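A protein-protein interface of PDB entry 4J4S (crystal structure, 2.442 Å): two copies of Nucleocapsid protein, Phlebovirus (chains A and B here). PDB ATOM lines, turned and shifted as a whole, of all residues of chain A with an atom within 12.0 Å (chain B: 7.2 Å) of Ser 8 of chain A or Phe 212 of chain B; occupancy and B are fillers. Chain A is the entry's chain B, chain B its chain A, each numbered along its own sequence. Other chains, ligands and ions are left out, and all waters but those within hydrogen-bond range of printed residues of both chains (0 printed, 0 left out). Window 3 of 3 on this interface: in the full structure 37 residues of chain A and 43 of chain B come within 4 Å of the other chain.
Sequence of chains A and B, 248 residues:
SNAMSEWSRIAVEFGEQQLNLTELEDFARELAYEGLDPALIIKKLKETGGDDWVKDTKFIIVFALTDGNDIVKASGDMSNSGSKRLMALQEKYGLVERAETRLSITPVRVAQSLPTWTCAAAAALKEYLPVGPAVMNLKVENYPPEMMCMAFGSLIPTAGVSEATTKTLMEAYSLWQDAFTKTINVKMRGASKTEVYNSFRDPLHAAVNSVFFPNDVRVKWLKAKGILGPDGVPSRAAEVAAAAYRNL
The side-chain carboxylate (OD1) of Asp 37 of chain B lies within hydrogen-bond range of the backbone NH (N) of Ala 39 of chain B. NE of Arg 218 of chain B lies within hydrogen-bond range of O of Phe 213 of chain B (2.8 Å). The backbone carbonyl oxygen (O) of Ala 3 of chain A sits at hydrogen-bond distance from the guanidinium group (NE) of Arg 9 of chain A (3.1 Å). OG of Ser 5 of chain A lies close to N of Trp 7 of chain A (3.5 Å). NE2 of Gln 17 of chain A sits at hydrogen-bond distance from O of Phe 14 of chain A, at 3.3 Å.
No position is printed for both chains.
The backbone carbonyl oxygen (O) of Phe 212 of chain B sits at hydrogen-bond distance from the side-chain hydroxyl (OG) of Ser 8 of chain A.
Of the printed residues of chain B, Trp 7 of chain A touches Ala 39, Ile 42 and Phe 212. Of chain B, only Phe 212 (2.8 Å) comes within 4 Å of Ser 8 of chain A. Of the printed residues of chain B, Phe 14 of chain A touches Leu 114 (3.6 Å). No residue of chain A comes within 4 Å of Pro 38 of chain B. Ala 39 of chain B touches just one residue of chain A: Trp 7. Printed residues of chain A within 4 Å of Ile 42 of chain B: Trp 7. Of the printed residues of chain A, Leu 114 of chain B touches Ala 11 (3.98 Å) and Phe 14 (3.6 Å). Pro 115 of chain B touches none of the printed residues of chain A. Ala 207 of chain B touches none of the printed residues of chain A. Of the printed residues of chain A, Pro 214 of chain B touches Ala 3.
Hydrophobic or aromatic side chains of chain B that line the printed part of chain A: Ala 39, Ile 42, Leu 114, Phe 212, Phe 213 and Pro 214. Of the 15 printed residues of chain A, 6 touch a printed residue of chain B. Hydrophobic or aromatic side chains of chain A within 4 Å of the printed part of chain B: Ala 3, Trp 7, Ala 11, Val 12 and Phe 14. Among the printed residues, no Asp or Glu carboxylate lies within 4 Å of a Lys or Arg side-chain nitrogen of the other chain.
Ala 3 of chain A touches Pro 214 of chain B. Ala 39 of chain B touches Trp 7 of chain A. Trp 7 of chain A touches Ile 42 of chain B. Phe 212 of chain B touches Trp 7 of chain A (CZ to O, 3.96 Å). Ser 113 of chain B touches Ala 11 of chain A (O to CB, 3.8 Å). Leu 114 of chain B touches Ala 11 of chain A. Ala 11 of chain A touches Phe 213 of chain B (CB to CE1, 3.9 Å). N of Val 12 of chain A touches CE1 of Phe 213 of chain B, 3.8 Å away. CG of Phe 14 of chain A touches CD1 of Leu 114 of chain B (3.6 Å).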
ATOM      1  N   ALA A   3       9.149  29.151 -19.606  1.00  0.00           N
ATOM      2  CA  ALA A   3       8.344  30.070 -18.805  1.00  0.00           C
ATOM      3  C   ALA A   3       8.574  29.974 -17.280  1.00  0.00           C
ATOM      4  O   ALA A   3       9.377  30.723 -16.726  1.00  0.00           O
ATOM      5  CB  ALA A   3       6.861  29.911 -19.128  1.00  0.00           C
ATOM      6  N   MET A   4       7.857  29.070 -16.611  1.00  0.00           N
ATOM      7  CA  MET A   4       7.805  29.037 -15.141  1.00  0.00           C
ATOM      8  C   MET A   4       9.065  28.525 -14.439  1.00  0.00           C
ATOM      9  O   MET A   4       9.270  28.790 -13.251  1.00  0.00           O
ATOM     10  CB  MET A   4       6.589  28.231 -14.654  1.00  0.00           C
ATOM     11  CG  MET A   4       5.261  28.921 -14.877  1.00  0.00           C
ATOM     12  SD  MET A   4       3.843  27.824 -14.675  1.00  0.00           S
ATOM     13  CE  MET A   4       2.715  28.529 -15.887  1.00  0.00           C
ATOM     14  N   SER A   5       9.896  27.783 -15.162  1.00  0.00           N
ATOM     15  CA  SER A   5      11.074  27.170 -14.567  1.00  0.00           C
ATOM     16  C   SER A   5      12.321  27.791 -15.171  1.00  0.00           C
ATOM     17  O   SER A   5      12.306  28.209 -16.325  1.00  0.00           O
ATOM     18  CB  SER A   5      11.058  25.669 -14.846  1.00  0.00           C
ATOM     19  OG  SER A   5      12.197  25.025 -14.322  1.00  0.00           O
ATOM     20  N   GLU A   6      13.407  27.860 -14.409  1.00  0.00           N
ATOM     21  CA  GLU A   6      14.621  28.442 -14.959  1.00  0.00           C
ATOM     22  C   GLU A   6      15.103  27.607 -16.151  1.00  0.00           C
ATOM     23  O   GLU A   6      15.638  28.149 -17.092  1.00  0.00           O
ATOM     24  CB  GLU A   6      15.727  28.592 -13.912  1.00  0.00           C
ATOM     25  CG  GLU A   6      16.372  27.289 -13.501  1.00  0.00           C
ATOM     26  CD  GLU A   6      17.777  27.477 -12.971  1.00  0.00           C
ATOM     27  OE1 GLU A   6      18.698  27.639 -13.805  1.00  0.00           O
ATOM     28  OE2 GLU A   6      17.959  27.466 -11.728  1.00  0.00           O
ATOM     29  N   TRP A   7      14.872  26.298 -16.103  1.00  0.00           N
ATOM     30  CA  TRP A   7      15.256  25.399 -17.174  1.00  0.00           C
ATOM     31  C   TRP A   7      14.373  25.578 -18.429  1.00  0.00           C
ATOM     32  O   TRP A   7      14.873  25.540 -19.569  1.00  0.00           O
ATOM     33  CB  TRP A   7      15.181  23.956 -16.685  1.00  0.00           C
ATOM     34  CG  TRP A   7      15.960  23.694 -15.427  1.00  0.00           C
ATOM     35  CD1 TRP A   7      15.448  23.358 -14.205  1.00  0.00           C
ATOM     36  CD2 TRP A   7      17.388  23.756 -15.258  1.00  0.00           C
ATOM     37  NE1 TRP A   7      16.460  23.199 -13.294  1.00  0.00           N
ATOM     38  CE2 TRP A   7      17.660  23.437 -13.912  1.00  0.00           C
ATOM     39  CE3 TRP A   7      18.459  24.039 -16.116  1.00  0.00           C
ATOM     40  CZ2 TRP A   7      18.958  23.398 -13.402  1.00  0.00           C
ATOM     41  CZ3 TRP A   7      19.747  23.999 -15.608  1.00  0.00           C
ATOM     42  CH2 TRP A   7      19.984  23.685 -14.263  1.00  0.00           C
ATOM     43  N   SER A   8      13.071  25.760 -18.212  1.00  0.00           N
ATOM     44  CA  SER A   8      12.147  26.101 -19.277  1.00  0.00           C
ATOM     45  C   SER A   8      12.589  27.401 -19.911  1.00  0.00           C
ATOM     46  O   SER A   8      12.646  27.501 -21.131  1.00  0.00           O
ATOM     47  CB  SER A   8      10.712  26.243 -18.765  1.00  0.00           C
ATOM     48  OG  SER A   8      10.174  24.986 -18.400  1.00  0.00           O
ATOM     49  N   ARG A   9      12.916  28.389 -19.085  1.00  0.00           N
ATOM     50  CA  ARG A   9      13.323  29.692 -19.596  1.00  0.00           C
ATOM     51  C   ARG A   9      14.557  29.538 -20.456  1.00  0.00           C
ATOM     52  O   ARG A   9      14.680  30.174 -21.506  1.00  0.00           O
ATOM     53  CB  ARG A   9      13.625  30.654 -18.455  1.00  0.00           C
ATOM     54  CG  ARG A   9      12.412  31.089 -17.682  1.00  0.00           C
ATOM     55  CD  ARG A   9      12.764  32.241 -16.775  1.00  0.00           C
ATOM     56  NE  ARG A   9      11.663  32.589 -15.890  1.00  0.00           N
ATOM     57  CZ  ARG A   9      11.556  32.159 -14.637  1.00  0.00           C
ATOM     58  NH1 ARG A   9      12.488  31.363 -14.116  1.00  0.00           N
ATOM     59  NH2 ARG A   9      10.516  32.531 -13.902  1.00  0.00           N
ATOM     60  N   ILE A  10      15.472  28.688 -19.994  1.00  0.00           N
ATOM     61  CA  ILE A  10      16.666  28.343 -20.757  1.00  0.00           C
ATOM     62  C   ILE A  10      16.312  27.753 -22.131  1.00  0.00           C
ATOM     63  O   ILE A  10      16.871  28.166 -23.152  1.00  0.00           O
ATOM     64  CB  ILE A  10      17.580  27.384 -19.970  1.00  0.00           C
ATOM     65  CG1 ILE A  10      18.176  28.114 -18.761  1.00  0.00           C
ATOM     66  CG2 ILE A  10      18.710  26.849 -20.875  1.00  0.00           C
ATOM     67  CD1 ILE A  10      18.943  27.214 -17.806  1.00  0.00           C
ATOM     68  N   ALA A  11      15.354  26.823 -22.150  1.00  0.00           N
ATOM     69  CA  ALA A  11      14.952  26.119 -23.378  1.00  0.00           C
ATOM     70  C   ALA A  11      14.405  27.055 -24.448  1.00  0.00           C
ATOM     71  O   ALA A  11      14.851  27.026 -25.604  1.00  0.00           O
ATOM     72  CB  ALA A  11      13.948  25.028 -23.063  1.00  0.00           C
ATOM     73  N   VAL A  12      13.475  27.919 -24.059  1.00  0.00           N
ATOM     74  CA  VAL A  12      12.925  28.877 -25.005  1.00  0.00           C
ATOM     75  C   VAL A  12      13.975  29.912 -25.401  1.00  0.00           C
ATOM     76  O   VAL A  12      14.087  30.264 -26.577  1.00  0.00           O
ATOM     77  CB  VAL A  12      11.579  29.497 -24.522  1.00  0.00           C
ATOM     78  CG1 VAL A  12      11.003  28.677 -23.390  1.00  0.00           C
ATOM     79  CG2 VAL A  12      11.722  30.957 -24.134  1.00  0.00           C
ATOM     80  N   GLU A  13      14.784  30.362 -24.448  1.00  0.00           N
ATOM     81  CA  GLU A  13      15.893  31.253 -24.803  1.00  0.00           C
ATOM     82  C   GLU A  13      16.878  30.617 -25.784  1.00  0.00           C
ATOM     83  O   GLU A  13      17.412  31.311 -26.650  1.00  0.00           O
ATOM     84  CB  GLU A  13      16.618  31.800 -23.572  1.00  0.00           C
ATOM     85  CG  GLU A  13      16.193  33.226 -23.242  1.00  0.00           C
ATOM     86  CD  GLU A  13      16.929  33.808 -22.056  1.00  0.00           C
ATOM     87  OE1 GLU A  13      18.184  33.800 -22.083  1.00  0.00           O
ATOM     88  OE2 GLU A  13      16.247  34.276 -21.105  1.00  0.00           O
ATOM     89  N   PHE A  14      17.117  29.310 -25.652  1.00  0.00           N
ATOM     90  CA  PHE A  14      17.996  28.570 -26.580  1.00  0.00           C
ATOM     91  C   PHE A  14      17.423  28.569 -28.015  1.00  0.00           C
ATOM     92  O   PHE A  14      18.172  28.605 -29.025  1.00  0.00           O
ATOM     93  CB  PHE A  14      18.138  27.139 -26.077  1.00  0.00           C
ATOM     94  CG  PHE A  14      19.339  26.429 -26.586  1.00  0.00           C
ATOM     95  CD1 PHE A  14      19.375  25.946 -27.880  1.00  0.00           C
ATOM     96  CD2 PHE A  14      20.435  26.212 -25.751  1.00  0.00           C
ATOM     97  CE1 PHE A  14      20.479  25.276 -28.352  1.00  0.00           C
ATOM     98  CE2 PHE A  14      21.525  25.535 -26.193  1.00  0.00           C
ATOM     99  CZ  PHE A  14      21.557  25.065 -27.509  1.00  0.00           C
ATOM    100  N   GLY A  15      16.089  28.549 -28.101  1.00  0.00           N
ATOM    101  CA  GLY A  15      15.414  28.569 -29.391  1.00  0.00           C
ATOM    102  C   GLY A  15      15.353  29.940 -30.039  1.00  0.00           C
ATOM    103  O   GLY A  15      15.005  30.050 -31.214  1.00  0.00           O
ATOM    104  N   GLU A  16      15.691  30.988 -29.289  1.00  0.00           N
ATOM    105  CA  GLU A  16      15.678  32.358 -29.823  1.00  0.00           C
ATOM    106  C   GLU A  16      17.036  32.785 -30.428  1.00  0.00           C
ATOM    107  O   GLU A  16      17.191  33.885 -30.977  1.00  0.00           O
ATOM    108  CB  GLU A  16      15.196  33.334 -28.744  1.00  0.00           C
ATOM    109  CG  GLU A  16      13.706  33.162 -28.397  1.00  0.00           C
ATOM    110  CD  GLU A  16      13.324  33.744 -27.032  1.00  0.00           C
ATOM    111  OE1 GLU A  16      14.240  34.179 -26.291  1.00  0.00           O
ATOM    112  OE2 GLU A  16      12.109  33.756 -26.698  1.00  0.00           O
ATOM    113  N   GLN A  17      18.014  31.890 -30.332  1.00  0.00           N
ATOM    114  CA  GLN A  17      19.334  32.150 -30.884  1.00  0.00           C
ATOM    115  C   GLN A  17      19.268  32.152 -32.387  1.00  0.00           C
ATOM    116  O   GLN A  17      18.715  31.232 -32.997  1.00  0.00           O
ATOM    117  CB  GLN A  17      20.321  31.052 -30.523  1.00  0.00           C
ATOM    118  CG  GLN A  17      20.618  30.828 -29.066  1.00  0.00           C
ATOM    119  CD  GLN A  17      21.682  29.734 -28.906  1.00  0.00           C
ATOM    120  OE1 GLN A  17      22.812  29.867 -29.424  1.00  0.00           O
ATOM    121  NE2 GLN A  17      21.327  28.645 -28.202  1.00  0.00           N
ATOM    122  N   LEU B  36      10.604  11.586 -21.414  1.00  0.00           N
ATOM    123  CA  LEU B  36      11.786  12.165 -20.921  1.00  0.00           C
ATOM    124  C   LEU B  36      11.466  13.303 -19.956  1.00  0.00           C
ATOM    125  O   LEU B  36      10.353  13.802 -19.991  1.00  0.00           O
ATOM    126  CB  LEU B  36      12.589  12.661 -22.099  1.00  0.00           C
ATOM    127  CG  LEU B  36      12.535  14.154 -22.195  1.00  0.00           C
ATOM    128  CD1 LEU B  36      13.037  14.637 -23.499  1.00  0.00           C
ATOM    129  CD2 LEU B  36      11.078  14.492 -22.061  1.00  0.00           C
ATOM    130  N   ASP B  37      12.427  13.649 -19.053  1.00  0.00           N
ATOM    131  CA  ASP B  37      12.371  14.884 -18.298  1.00  0.00           C
ATOM    132  C   ASP B  37      13.332  15.887 -18.917  1.00  0.00           C
ATOM    133  O   ASP B  37      14.528  15.766 -18.746  1.00  0.00           O
ATOM    134  CB  ASP B  37      12.754  14.655 -16.842  1.00  0.00           C
ATOM    135  CG  ASP B  37      12.246  15.759 -15.942  1.00  0.00           C
ATOM    136  OD1 ASP B  37      12.308  16.944 -16.366  1.00  0.00           O
ATOM    137  OD2 ASP B  37      11.752  15.437 -14.838  1.00  0.00           O
ATOM    138  N   PRO B  38      12.812  16.895 -19.625  1.00  0.00           N
ATOM    139  CA  PRO B  38      13.776  17.806 -20.262  1.00  0.00           C
ATOM    140  C   PRO B  38      14.556  18.703 -19.277  1.00  0.00           C
ATOM    141  O   PRO B  38      15.730  19.012 -19.535  1.00  0.00           O
ATOM    142  CB  PRO B  38      12.913  18.652 -21.215  1.00  0.00           C
ATOM    143  CG  PRO B  38      11.522  18.008 -21.200  1.00  0.00           C
ATOM    144  CD  PRO B  38      11.403  17.217 -19.940  1.00  0.00           C
ATOM    145  N   ALA B  39      13.933  19.111 -18.173  1.00  0.00           N
ATOM    146  CA  ALA B  39      14.577  20.064 -17.261  1.00  0.00           C
ATOM    147  C   ALA B  39      15.886  19.519 -16.698  1.00  0.00           C
ATOM    148  O   ALA B  39      16.843  20.258 -16.473  1.00  0.00           O
ATOM    149  CB  ALA B  39      13.646  20.448 -16.136  1.00  0.00           C
ATOM    150  N   LEU B  40      15.925  18.213 -16.480  1.00  0.00           N
ATOM    151  CA  LEU B  40      17.089  17.588 -15.885  1.00  0.00           C
ATOM    152  C   LEU B  40      18.115  17.156 -16.941  1.00  0.00           C
ATOM    153  O   LEU B  40      19.291  16.969 -16.628  1.00  0.00           O
ATOM    154  CB  LEU B  40      16.635  16.427 -15.001  1.00  0.00           C
ATOM    155  CG  LEU B  40      16.957  14.980 -15.354  1.00  0.00           C
ATOM    156  CD1 LEU B  40      18.323  14.624 -14.803  1.00  0.00           C
ATOM    157  CD2 LEU B  40      15.874  14.050 -14.793  1.00  0.00           C
ATOM    158  N   ILE B  42      18.685  19.161 -19.430  1.00  0.00           N
ATOM    159  CA  ILE B  42      19.320  20.447 -19.664  1.00  0.00           C
ATOM    160  C   ILE B  42      20.356  20.730 -18.568  1.00  0.00           C
ATOM    161  O   ILE B  42      21.515  21.033 -18.870  1.00  0.00           O
ATOM    162  CB  ILE B  42      18.272  21.561 -19.787  1.00  0.00           C
ATOM    163  CG1 ILE B  42      17.421  21.329 -21.038  1.00  0.00           C
ATOM    164  CG2 ILE B  42      18.908  22.917 -19.898  1.00  0.00           C
ATOM    165  CD1 ILE B  42      16.240  22.272 -21.160  1.00  0.00           C
ATOM    166  N   GLN B 112      14.917  17.126 -28.185  1.00  0.00           N
ATOM    167  CA  GLN B 112      13.600  17.321 -27.656  1.00  0.00           C
ATOM    168  C   GLN B 112      13.507  18.287 -26.557  1.00  0.00           C
ATOM    169  O   GLN B 112      12.527  18.930 -26.365  1.00  0.00           O
ATOM    170  CB  GLN B 112      13.090  16.025 -27.214  1.00  0.00           C
ATOM    171  CG  GLN B 112      13.059  15.121 -28.366  1.00  0.00           C
ATOM    172  CD  GLN B 112      12.620  13.791 -27.967  1.00  0.00           C
ATOM    173  OE1 GLN B 112      12.883  13.362 -26.877  1.00  0.00           O
ATOM    174  NE2 GLN B 112      11.933  13.124 -28.834  1.00  0.00           N
ATOM    175  N   SER B 113      14.515  18.327 -25.754  1.00  0.00           N
ATOM    176  CA  SER B 113      14.489  19.235 -24.679  1.00  0.00           C
ATOM    177  C   SER B 113      14.724  20.601 -25.133  1.00  0.00           C
ATOM    178  O   SER B 113      14.466  21.513 -24.442  1.00  0.00           O
ATOM    179  CB  SER B 113      15.470  18.786 -23.648  1.00  0.00           C
ATOM    180  OG  SER B 113      15.604  17.406 -23.768  1.00  0.00           O
ATOM    181  N   LEU B 114      15.215  20.762 -26.334  1.00  0.00           N
ATOM    182  CA  LEU B 114      15.414  22.103 -26.823  1.00  0.00           C
ATOM    183  C   LEU B 114      14.735  22.191 -28.139  1.00  0.00           C
ATOM    184  O   LEU B 114      15.381  22.392 -29.113  1.00  0.00           O
ATOM    185  CB  LEU B 114      16.877  22.366 -27.096  1.00  0.00           C
ATOM    186  CG  LEU B 114      17.991  22.764 -26.145  1.00  0.00           C
ATOM    187  CD1 LEU B 114      17.627  23.676 -25.019  1.00  0.00           C
ATOM    188  CD2 LEU B 114      18.772  21.580 -25.678  1.00  0.00           C
ATOM    189  N   PRO B 115      13.417  22.062 -28.124  1.00  0.00           N
ATOM    190  CA  PRO B 115      12.547  21.886 -29.270  1.00  0.00           C
ATOM    191  C   PRO B 115      12.435  23.053 -30.244  1.00  0.00           C
ATOM    192  O   PRO B 115      12.297  22.830 -31.393  1.00  0.00           O
ATOM    193  CB  PRO B 115      11.250  21.678 -28.591  1.00  0.00           C
ATOM    194  CG  PRO B 115      11.318  22.710 -27.588  1.00  0.00           C
ATOM    195  CD  PRO B 115      12.635  22.532 -26.991  1.00  0.00           C
ATOM    196  N   ALA B 207       4.675  14.326 -25.468  1.00  0.00           N
ATOM    197  CA  ALA B 207       5.246  15.592 -25.895  1.00  0.00           C
ATOM    198  C   ALA B 207       4.172  16.656 -25.994  1.00  0.00           C
ATOM    199  O   ALA B 207       4.345  17.779 -25.526  1.00  0.00           O
ATOM    200  CB  ALA B 207       5.984  15.434 -27.211  1.00  0.00           C
ATOM    201  N   ASN B 209       1.268  16.744 -24.525  1.00  0.00           N
ATOM    202  CA  ASN B 209       0.657  16.985 -23.219  1.00  0.00           C
ATOM    203  C   ASN B 209       1.590  17.525 -22.144  1.00  0.00           C
ATOM    204  O   ASN B 209       1.145  17.913 -21.060  1.00  0.00           O
ATOM    205  CB  ASN B 209       0.029  15.693 -22.690  1.00  0.00           C
ATOM    206  CG  ASN B 209      -1.235  15.309 -23.440  1.00  0.00           C
ATOM    207  OD1 ASN B 209      -1.811  16.126 -24.159  1.00  0.00           O
ATOM    208  ND2 ASN B 209      -1.678  14.060 -23.262  1.00  0.00           N
ATOM    209  N   SER B 210       2.889  17.525 -22.417  1.00  0.00           N
ATOM    210  CA  SER B 210       3.833  17.976 -21.406  1.00  0.00           C
ATOM    211  C   SER B 210       3.650  19.479 -21.167  1.00  0.00           C
ATOM    212  O   SER B 210       3.282  20.222 -22.081  1.00  0.00           O
ATOM    213  CB  SER B 210       5.274  17.650 -21.822  1.00  0.00           C
ATOM    214  OG  SER B 210       5.841  18.726 -22.538  1.00  0.00           O
ATOM    215  N   VAL B 211       3.898  19.915 -19.936  1.00  0.00           N
ATOM    216  CA  VAL B 211       3.790  21.329 -19.581  1.00  0.00           C
ATOM    217  C   VAL B 211       5.149  22.019 -19.539  1.00  0.00           C
ATOM    218  O   VAL B 211       5.224  23.244 -19.388  1.00  0.00           O
ATOM    219  CB  VAL B 211       3.106  21.523 -18.212  1.00  0.00           C
ATOM    220  CG1 VAL B 211       1.611  21.309 -18.336  1.00  0.00           C
ATOM    221  CG2 VAL B 211       3.711  20.573 -17.188  1.00  0.00           C
ATOM    222  N   PHE B 212       6.219  21.240 -19.666  1.00  0.00           N
ATOM    223  CA  PHE B 212       7.556  21.802 -19.600  1.00  0.00           C
ATOM    224  C   PHE B 212       7.767  22.971 -20.569  1.00  0.00           C
ATOM    225  O   PHE B 212       8.129  24.071 -20.145  1.00  0.00           O
ATOM    226  CB  PHE B 212       8.611  20.733 -19.822  1.00  0.00           C
ATOM    227  CG  PHE B 212       9.994  21.282 -19.863  1.00  0.00           C
ATOM    228  CD1 PHE B 212      10.614  21.725 -18.696  1.00  0.00           C
ATOM    229  CD2 PHE B 212      10.666  21.396 -21.063  1.00  0.00           C
ATOM    230  CE1 PHE B 212      11.888  22.253 -18.736  1.00  0.00           C
ATOM    231  CE2 PHE B 212      11.954  21.918 -21.110  1.00  0.00           C
ATOM    232  CZ  PHE B 212      12.564  22.347 -19.950  1.00  0.00           C
ATOM    233  N   PHE B 213       7.535  22.742 -21.862  1.00  0.00           N
ATOM    234  CA  PHE B 213       7.650  23.824 -22.836  1.00  0.00           C
ATOM    235  C   PHE B 213       6.307  24.544 -23.002  1.00  0.00           C
ATOM    236  O   PHE B 213       5.350  23.974 -23.528  1.00  0.00           O
ATOM    237  CB  PHE B 213       8.155  23.298 -24.176  1.00  0.00           C
ATOM    238  CG  PHE B 213       8.886  24.325 -24.977  1.00  0.00           C
ATOM    239  CD1 PHE B 213      10.260  24.490 -24.823  1.00  0.00           C
ATOM    240  CD2 PHE B 213       8.207  25.147 -25.864  1.00  0.00           C
ATOM    241  CE1 PHE B 213      10.940  25.445 -25.553  1.00  0.00           C
ATOM    242  CE2 PHE B 213       8.872  26.105 -26.589  1.00  0.00           C
ATOM    243  CZ  PHE B 213      10.245  26.256 -26.439  1.00  0.00           C
ATOM    244  N   PRO B 214       6.247  25.814 -22.574  1.00  0.00           N
ATOM    245  CA  PRO B 214       4.986  26.547 -22.388  1.00  0.00           C
ATOM    246  C   PRO B 214       4.169  26.709 -23.663  1.00  0.00           C
ATOM    247  O   PRO B 214       4.719  26.938 -24.736  1.00  0.00           O
ATOM    248  CB  PRO B 214       5.440  27.909 -21.836  1.00  0.00           C
ATOM    249  CG  PRO B 214       6.852  28.040 -22.233  1.00  0.00           C
ATOM    250  CD  PRO B 214       7.431  26.664 -22.370  1.00  0.00           C
ATOM    251  N   ASN B 215       2.854  26.596 -23.532  1.00  0.00           N
ATOM    252  CA  ASN B 215       1.966  26.607 -24.688  1.00  0.00           C
ATOM    253  C   ASN B 215       1.956  27.914 -25.484  1.00  0.00           C
ATOM    254  O   ASN B 215       1.927  27.883 -26.704  1.00  0.00           O
ATOM    255  CB  ASN B 215       0.544  26.165 -24.302  1.00  0.00           C
ATOM    256  CG  ASN B 215       0.357  24.649 -24.396  1.00  0.00           C
ATOM    257  OD1 ASN B 215       0.352  24.085 -25.485  1.00  0.00           O
ATOM    258  ND2 ASN B 215       0.194  23.995 -23.261  1.00  0.00           N
ATOM    259  N   ARG B 218       4.759  27.946 -27.923  1.00  0.00           N
ATOM    260  CA  ARG B 218       4.508  27.011 -29.024  1.00  0.00           C
ATOM    261  C   ARG B 218       3.636  27.706 -30.088  1.00  0.00           C
ATOM    262  O   ARG B 218       3.940  27.667 -31.281  1.00  0.00           O
ATOM    263  CB  ARG B 218       3.810  25.739 -28.550  1.00  0.00           C
ATOM    264  CG  ARG B 218       4.470  24.996 -27.432  1.00  0.00           C
ATOM    265  CD  ARG B 218       3.714  23.704 -27.168  1.00  0.00           C
ATOM    266  NE  ARG B 218       4.059  23.141 -25.875  1.00  0.00           N
ATOM    267  CZ  ARG B 218       3.647  21.956 -25.437  1.00  0.00           C
ATOM    268  NH1 ARG B 218       2.870  21.203 -26.207  1.00  0.00           N
ATOM    269  NH2 ARG B 218       4.023  21.516 -24.228  1.00  0.00           N
